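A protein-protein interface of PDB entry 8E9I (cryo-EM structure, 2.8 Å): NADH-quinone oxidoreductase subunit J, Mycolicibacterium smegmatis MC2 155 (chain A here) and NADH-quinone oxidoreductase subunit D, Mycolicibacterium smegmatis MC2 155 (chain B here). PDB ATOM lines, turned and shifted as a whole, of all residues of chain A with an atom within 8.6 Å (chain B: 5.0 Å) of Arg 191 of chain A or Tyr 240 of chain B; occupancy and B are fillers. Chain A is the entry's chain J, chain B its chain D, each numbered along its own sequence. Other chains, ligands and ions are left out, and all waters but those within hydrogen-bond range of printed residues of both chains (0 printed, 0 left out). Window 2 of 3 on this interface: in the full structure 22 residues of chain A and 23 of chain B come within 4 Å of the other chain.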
ATOM      1  N   LYS A 188      17.114  -7.651 -20.466  1.00  0.00           N
ATOM      2  CA  LYS A 188      17.979  -6.505 -20.230  1.00  0.00           C
ATOM      3  C   LYS A 188      18.798  -6.198 -21.478  1.00  0.00           C
ATOM      4  O   LYS A 188      19.185  -7.104 -22.222  1.00  0.00           O
ATOM      5  CB  LYS A 188      18.899  -6.770 -19.040  1.00  0.00           C
ATOM      6  N   THR A 189      19.051  -4.916 -21.710  1.00  0.00           N
ATOM      7  CA  THR A 189      19.856  -4.503 -22.849  1.00  0.00           C
ATOM      8  C   THR A 189      21.335  -4.716 -22.554  1.00  0.00           C
ATOM      9  O   THR A 189      21.762  -4.743 -21.397  1.00  0.00           O
ATOM     10  CB  THR A 189      19.599  -3.032 -23.171  1.00  0.00           C
ATOM     11  OG1 THR A 189      18.189  -2.794 -23.234  1.00  0.00           O
ATOM     12  CG2 THR A 189      20.211  -2.666 -24.507  1.00  0.00           C
ATOM     13  N   GLN A 190      22.125  -4.866 -23.619  1.00  0.00           N
ATOM     14  CA  GLN A 190      23.572  -4.902 -23.448  1.00  0.00           C
ATOM     15  C   GLN A 190      24.041  -3.706 -22.635  1.00  0.00           C
ATOM     16  O   GLN A 190      24.872  -3.841 -21.724  1.00  0.00           O
ATOM     17  CB  GLN A 190      24.258  -4.919 -24.812  1.00  0.00           C
ATOM     18  CG  GLN A 190      25.768  -5.042 -24.751  1.00  0.00           C
ATOM     19  CD  GLN A 190      26.470  -3.707 -24.721  1.00  0.00           C
ATOM     20  OE1 GLN A 190      26.252  -2.856 -25.578  1.00  0.00           O
ATOM     21  NE2 GLN A 190      27.323  -3.516 -23.729  1.00  0.00           N
ATOM     22  N   ARG A 191      23.511  -2.526 -22.951  1.00  0.00           N
ATOM     23  CA  ARG A 191      23.796  -1.338 -22.161  1.00  0.00           C
ATOM     24  C   ARG A 191      23.463  -1.580 -20.699  1.00  0.00           C
ATOM     25  O   ARG A 191      24.263  -1.285 -19.805  1.00  0.00           O
ATOM     26  CB  ARG A 191      22.994  -0.159 -22.703  1.00  0.00           C
ATOM     27  CG  ARG A 191      23.289   1.145 -22.017  1.00  0.00           C
ATOM     28  CD  ARG A 191      22.386   2.250 -22.520  1.00  0.00           C
ATOM     29  NE  ARG A 191      23.007   3.560 -22.393  1.00  0.00           N
ATOM     30  CZ  ARG A 191      23.140   4.213 -21.248  1.00  0.00           C
ATOM     31  NH1 ARG A 191      22.764   3.677 -20.098  1.00  0.00           N
ATOM     32  NH2 ARG A 191      23.673   5.430 -21.254  1.00  0.00           N
ATOM     33  N   GLU A 192      22.279  -2.129 -20.437  1.00  0.00           N
ATOM     34  CA  GLU A 192      21.883  -2.403 -19.064  1.00  0.00           C
ATOM     35  C   GLU A 192      22.826  -3.410 -18.424  1.00  0.00           C
ATOM     36  O   GLU A 192      23.199  -3.277 -17.254  1.00  0.00           O
ATOM     37  CB  GLU A 192      20.441  -2.912 -19.032  1.00  0.00           C
ATOM     38  N   LEU A 193      23.227  -4.428 -19.185  1.00  0.00           N
ATOM     39  CA  LEU A 193      24.028  -5.501 -18.608  1.00  0.00           C
ATOM     40  C   LEU A 193      25.404  -5.009 -18.183  1.00  0.00           C
ATOM     41  O   LEU A 193      25.890  -5.371 -17.106  1.00  0.00           O
ATOM     42  CB  LEU A 193      24.152  -6.652 -19.604  1.00  0.00           C
ATOM     43  CG  LEU A 193      22.954  -7.600 -19.640  1.00  0.00           C
ATOM     44  CD1 LEU A 193      23.138  -8.631 -20.723  1.00  0.00           C
ATOM     45  CD2 LEU A 193      22.771  -8.276 -18.301  1.00  0.00           C
ATOM     46  N   ALA A 194      26.053  -4.187 -19.010  1.00  0.00           N
ATOM     47  CA  ALA A 194      27.398  -3.732 -18.664  1.00  0.00           C
ATOM     48  C   ALA A 194      27.415  -3.005 -17.319  1.00  0.00           C
ATOM     49  O   ALA A 194      28.413  -3.048 -16.592  1.00  0.00           O
ATOM     50  CB  ALA A 194      27.944  -2.833 -19.771  1.00  0.00           C
ATOM     51  N   ILE A 195      26.324  -2.324 -16.988  1.00  0.00           N
ATOM     52  CA  ILE A 195      26.141  -1.541 -15.766  1.00  0.00           C
ATOM     53  C   ILE A 195      25.801  -2.463 -14.591  1.00  0.00           C
ATOM     54  O   ILE A 195      25.785  -3.689 -14.741  1.00  0.00           O
ATOM     55  CB  ILE A 195      25.073  -0.452 -16.003  1.00  0.00           C
ATOM     56  CG1 ILE A 195      25.407   0.333 -17.279  1.00  0.00           C
ATOM     57  CG2 ILE A 195      24.996   0.527 -14.850  1.00  0.00           C
ATOM     58  CD1 ILE A 195      24.299   1.221 -17.768  1.00  0.00           C
ATOM     59  N   GLU A 196      25.571  -1.880 -13.404  1.00  0.00           N
ATOM     60  CA  GLU A 196      25.215  -2.606 -12.183  1.00  0.00           C
ATOM     61  C   GLU A 196      26.381  -3.322 -11.511  1.00  0.00           C
ATOM     62  O   GLU A 196      26.432  -4.555 -11.467  1.00  0.00           O
ATOM     63  CB  GLU A 196      24.111  -3.621 -12.494  1.00  0.00           C
ATOM     64  N   PHE A 198      29.365  -2.873 -12.626  1.00  0.00           N
ATOM     65  CA  PHE A 198      30.042  -3.328 -13.828  1.00  0.00           C
ATOM     66  C   PHE A 198      29.793  -4.814 -14.037  1.00  0.00           C
ATOM     67  O   PHE A 198      30.706  -5.631 -13.896  1.00  0.00           O
ATOM     68  CB  PHE A 198      31.534  -3.043 -13.750  1.00  0.00           C
ATOM     69  CG  PHE A 198      32.271  -3.433 -14.985  1.00  0.00           C
ATOM     70  CD1 PHE A 198      31.736  -3.169 -16.233  1.00  0.00           C
ATOM     71  CD2 PHE A 198      33.483  -4.075 -14.906  1.00  0.00           C
ATOM     72  CE1 PHE A 198      32.404  -3.529 -17.369  1.00  0.00           C
ATOM     73  CE2 PHE A 198      34.151  -4.437 -16.038  1.00  0.00           C
ATOM     74  CZ  PHE A 198      33.609  -4.165 -17.273  1.00  0.00           C
ATOM     75  N   GLN A 199      28.554  -5.174 -14.344  1.00  0.00           N
ATOM     76  CA  GLN A 199      28.204  -6.560 -14.579  1.00  0.00           C
ATOM     77  C   GLN A 199      28.908  -7.079 -15.833  1.00  0.00           C
ATOM     78  O   GLN A 199      29.217  -6.334 -16.765  1.00  0.00           O
ATOM     79  CB  GLN A 199      26.688  -6.706 -14.696  1.00  0.00           C
ATOM     80  N   THR A 200      29.182  -8.383 -15.838  1.00  0.00           N
ATOM     81  CA  THR A 200      29.729  -9.102 -16.985  1.00  0.00           C
ATOM     82  C   THR A 200      31.203  -8.816 -17.230  1.00  0.00           C
ATOM     83  O   THR A 200      31.827  -9.495 -18.050  1.00  0.00           O
ATOM     84  CB  THR A 200      28.949  -8.771 -18.262  1.00  0.00           C
ATOM     85  OG1 THR A 200      29.299  -7.456 -18.707  1.00  0.00           O
ATOM     86  CG2 THR A 200      27.445  -8.856 -18.032  1.00  0.00           C
ATOM     87  N   GLY B 237      24.988   3.211 -30.168  1.00  0.00           N
ATOM     88  CA  GLY B 237      24.430   2.546 -29.009  1.00  0.00           C
ATOM     89  C   GLY B 237      24.920   1.122 -28.864  1.00  0.00           C
ATOM     90  O   GLY B 237      24.577   0.435 -27.898  1.00  0.00           O
ATOM     91  N   VAL B 238      25.727   0.670 -29.820  1.00  0.00           N
ATOM     92  CA  VAL B 238      26.170  -0.716 -29.846  1.00  0.00           C
ATOM     93  C   VAL B 238      27.518  -0.829 -29.153  1.00  0.00           C
ATOM     94  O   VAL B 238      28.376   0.052 -29.281  1.00  0.00           O
ATOM     95  CB  VAL B 238      26.245  -1.222 -31.292  1.00  0.00           C
ATOM     96  CG1 VAL B 238      26.934  -2.569 -31.348  1.00  0.00           C
ATOM     97  CG2 VAL B 238      24.856  -1.288 -31.903  1.00  0.00           C
ATOM     98  N   GLY B 239      27.719  -1.924 -28.428  1.00  0.00           N
ATOM     99  CA  GLY B 239      28.956  -2.105 -27.697  1.00  0.00           C
ATOM    100  C   GLY B 239      29.159  -1.091 -26.599  1.00  0.00           C
ATOM    101  O   GLY B 239      30.294  -0.683 -26.341  1.00  0.00           O
ATOM    102  N   TYR B 240      28.084  -0.673 -25.943  1.00  0.00           N
ATOM    103  CA  TYR B 240      28.184   0.328 -24.895  1.00  0.00           C
ATOM    104  C   TYR B 240      29.075  -0.173 -23.772  1.00  0.00           C
ATOM    105  O   TYR B 240      29.016  -1.342 -23.386  1.00  0.00           O
ATOM    106  CB  TYR B 240      26.792   0.647 -24.360  1.00  0.00           C
ATOM    107  CG  TYR B 240      26.750   1.656 -23.242  1.00  0.00           C
ATOM    108  CD1 TYR B 240      27.001   1.279 -21.933  1.00  0.00           C
ATOM    109  CD2 TYR B 240      26.421   2.979 -23.491  1.00  0.00           C
ATOM    110  CE1 TYR B 240      26.952   2.191 -20.910  1.00  0.00           C
ATOM    111  CE2 TYR B 240      26.365   3.899 -22.472  1.00  0.00           C
ATOM    112  CZ  TYR B 240      26.631   3.499 -21.184  1.00  0.00           C
ATOM    113  OH  TYR B 240      26.577   4.415 -20.162  1.00  0.00           O
ATOM    114  N   LEU B 241      29.909   0.718 -23.247  1.00  0.00           N
ATOM    115  CA  LEU B 241      30.796   0.390 -22.140  1.00  0.00           C
ATOM    116  C   LEU B 241      30.971   1.633 -21.287  1.00  0.00           C
ATOM    117  O   LEU B 241      31.434   2.664 -21.782  1.00  0.00           O
ATOM    118  CB  LEU B 241      32.149  -0.113 -22.645  1.00  0.00           C
ATOM    119  CG  LEU B 241      33.153  -0.523 -21.572  1.00  0.00           C
ATOM    120  CD1 LEU B 241      32.673  -1.763 -20.840  1.00  0.00           C
ATOM    121  CD2 LEU B 241      34.506  -0.757 -22.196  1.00  0.00           C
ATOM    122  N   ASP B 242      30.602   1.536 -20.015  1.00  0.00           N
ATOM    123  CA  ASP B 242      30.665   2.688 -19.134  1.00  0.00           C
ATOM    124  C   ASP B 242      32.110   3.028 -18.795  1.00  0.00           C
ATOM    125  O   ASP B 242      33.005   2.183 -18.839  1.00  0.00           O
ATOM    126  CB  ASP B 242      29.884   2.424 -17.848  1.00  0.00           C
ATOM    127  N   ARG B 286      29.379   9.148 -26.494  1.00  0.00           N
ATOM    128  CA  ARG B 286      28.432   8.082 -26.793  1.00  0.00           C
ATOM    129  C   ARG B 286      28.718   6.807 -26.012  1.00  0.00           C
ATOM    130  O   ARG B 286      27.780   6.068 -25.701  1.00  0.00           O
ATOM    131  CB  ARG B 286      28.439   7.798 -28.293  1.00  0.00           C
ATOM    132  CG  ARG B 286      27.855   8.927 -29.120  1.00  0.00           C
ATOM    133  CD  ARG B 286      27.970   8.646 -30.600  1.00  0.00           C
ATOM    134  NE  ARG B 286      27.447   9.732 -31.418  1.00  0.00           N
ATOM    135  CZ  ARG B 286      28.084  10.872 -31.648  1.00  0.00           C
ATOM    136  NH1 ARG B 286      29.245  11.143 -31.078  1.00  0.00           N
ATOM    137  NH2 ARG B 286      27.536  11.766 -32.464  1.00  0.00           N
ATOM    138  N   CYS B 287      29.978   6.532 -25.688  1.00  0.00           N
ATOM    139  CA  CYS B 287      30.387   5.356 -24.924  1.00  0.00           C
ATOM    140  C   CYS B 287      30.109   4.051 -25.654  1.00  0.00           C
ATOM    141  O   CYS B 287      29.989   3.005 -25.009  1.00  0.00           O
ATOM    142  CB  CYS B 287      29.706   5.310 -23.552  1.00  0.00           C
ATOM    143  SG  CYS B 287      29.897   6.787 -22.551  1.00  0.00           S
ATOM    144  N   ASP B 288      29.997   4.078 -26.974  1.00  0.00           N
ATOM    145  CA  ASP B 288      29.577   2.925 -27.756  1.00  0.00           C
ATOM    146  C   ASP B 288      30.461   2.780 -28.987  1.00  0.00           C
ATOM    147  O   ASP B 288      31.480   3.453 -29.131  1.00  0.00           O
ATOM    148  CB  ASP B 288      28.107   3.057 -28.153  1.00  0.00           C
ATOM    149  CG  ASP B 288      27.831   4.311 -28.947  1.00  0.00           C
ATOM    150  OD1 ASP B 288      28.784   4.890 -29.505  1.00  0.00           O
ATOM    151  OD2 ASP B 288      26.654   4.721 -29.016  1.00  0.00           O
ATOM    152  N   ARG B 292      33.412   5.354 -30.626  1.00  0.00           N
ATOM    153  CA  ARG B 292      34.783   4.932 -30.872  1.00  0.00           C
ATOM    154  C   ARG B 292      35.169   5.165 -32.328  1.00  0.00           C
ATOM    155  O   ARG B 292      36.280   5.618 -32.628  1.00  0.00           O
ATOM    156  CB  ARG B 292      34.933   3.462 -30.488  1.00  0.00           C
ATOM    157  CG  ARG B 292      34.756   3.233 -28.999  1.00  0.00           C
ATOM    158  CD  ARG B 292      34.961   1.787 -28.606  1.00  0.00           C
ATOM    159  NE  ARG B 292      33.812   0.940 -28.892  1.00  0.00           N
ATOM    160  CZ  ARG B 292      32.836   0.686 -28.031  1.00  0.00           C
ATOM    161  NH1 ARG B 292      32.811   1.232 -26.827  1.00  0.00           N
ATOM    162  NH2 ARG B 292      31.859  -0.140 -28.389  1.00  0.00           N
ATOM    163  N   ALA B 416      31.698  -7.516 -21.889  1.00  0.00           N
ATOM    164  CA  ALA B 416      30.881  -6.354 -21.568  1.00  0.00           C
ATOM    165  C   ALA B 416      30.137  -5.830 -22.787  1.00  0.00           C
ATOM    166  O   ALA B 416      28.952  -5.492 -22.706  1.00  0.00           O
ATOM    167  CB  ALA B 416      31.764  -5.258 -20.973  1.00  0.00           C
ATOM    168  N   THR B 417      30.814  -5.758 -23.929  1.00  0.00           N
ATOM    169  CA  THR B 417      30.239  -5.101 -25.096  1.00  0.00           C
ATOM    170  C   THR B 417      29.460  -6.044 -25.997  1.00  0.00           C
ATOM    171  O   THR B 417      28.780  -5.573 -26.914  1.00  0.00           O
ATOM    172  CB  THR B 417      31.341  -4.429 -25.911  1.00  0.00           C
ATOM    173  OG1 THR B 417      32.322  -5.402 -26.287  1.00  0.00           O
ATOM    174  CG2 THR B 417      32.000  -3.336 -25.105  1.00  0.00           C
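Gln 190 of chain A touches Thr 417 of chain B. CD1 of Leu 241 of chain B touches CE1 of Phe 198 of chain A (3.9 Å). Thr 200 of chain A touches Ala 416 of chain B.
The guanidinium group of Arg 292 of chain B is in hydrogen-bond range of the backbone carbonyl oxygen of Gly 239 of chain B (2.6 Å). The backbone NH (N) of Leu 241 of chain B is in hydrogen-bond range of the backbone carbonyl oxygen (O) of Cys 287 of chain B.
Of chain B, only Tyr 240 comes within 4 Å of Arg 191 of chain A. Tyr 240 of chain B touches two residues of chain A. Gly 239 of chain B touches one residue of chain A. Printed residues of chain A within 4 Å of Leu 241 of chain B: Phe 198 (3.9 Å). Printed residues of chain B within 4 Å of Phe 198 of chain A: Leu 241 (3.9 Å). Of the printed residues of chain A, Thr 417 of chain B touches Gln 190. Of the printed residues of chain B, Gln 190 of chain A touches Gly 239, Tyr 240, Ala 416 and Thr 417. Gln 199 of chain A touches none of the printed residues of chain B. The nearest residue of chain A that does not touch Tyr 240 of chain B is Ala 194 of chain A (4.1 Å).
Hydrophobic or aromatic side chains of chain B within 4 Å of the printed part of chain A: Tyr 240 and Leu 241. Along chain B the printed residues that touch a printed residue of chain A span positions 239 to 417. Among the printed residues, no Asp or Glu carboxylate lies within 4 Å of a Lys or Arg side-chain nitrogen of the other chain.
The side-chain amide oxygen (OE1) of Gln 190 of chain A lies within hydrogen-bond range of the backbone NH (N) of Gly 239 of chain B, at 3.3 Å. NE2 of Gln 190 of chain A is in hydrogen-bond range of O of Tyr 240 of chain B (2.8 Å). The backbone carbonyl oxygen (O) of Ala 416 of chain B sits at hydrogen-bond distance from the side-chain amide nitrogen (NE2) of Gln 190 of chain A (2.8 Å). The guanidinium group of Arg 191 of chain A lies within hydrogen-bond range of the side-chain hydroxyl of Tyr 240 of chain B (3.3 Å).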
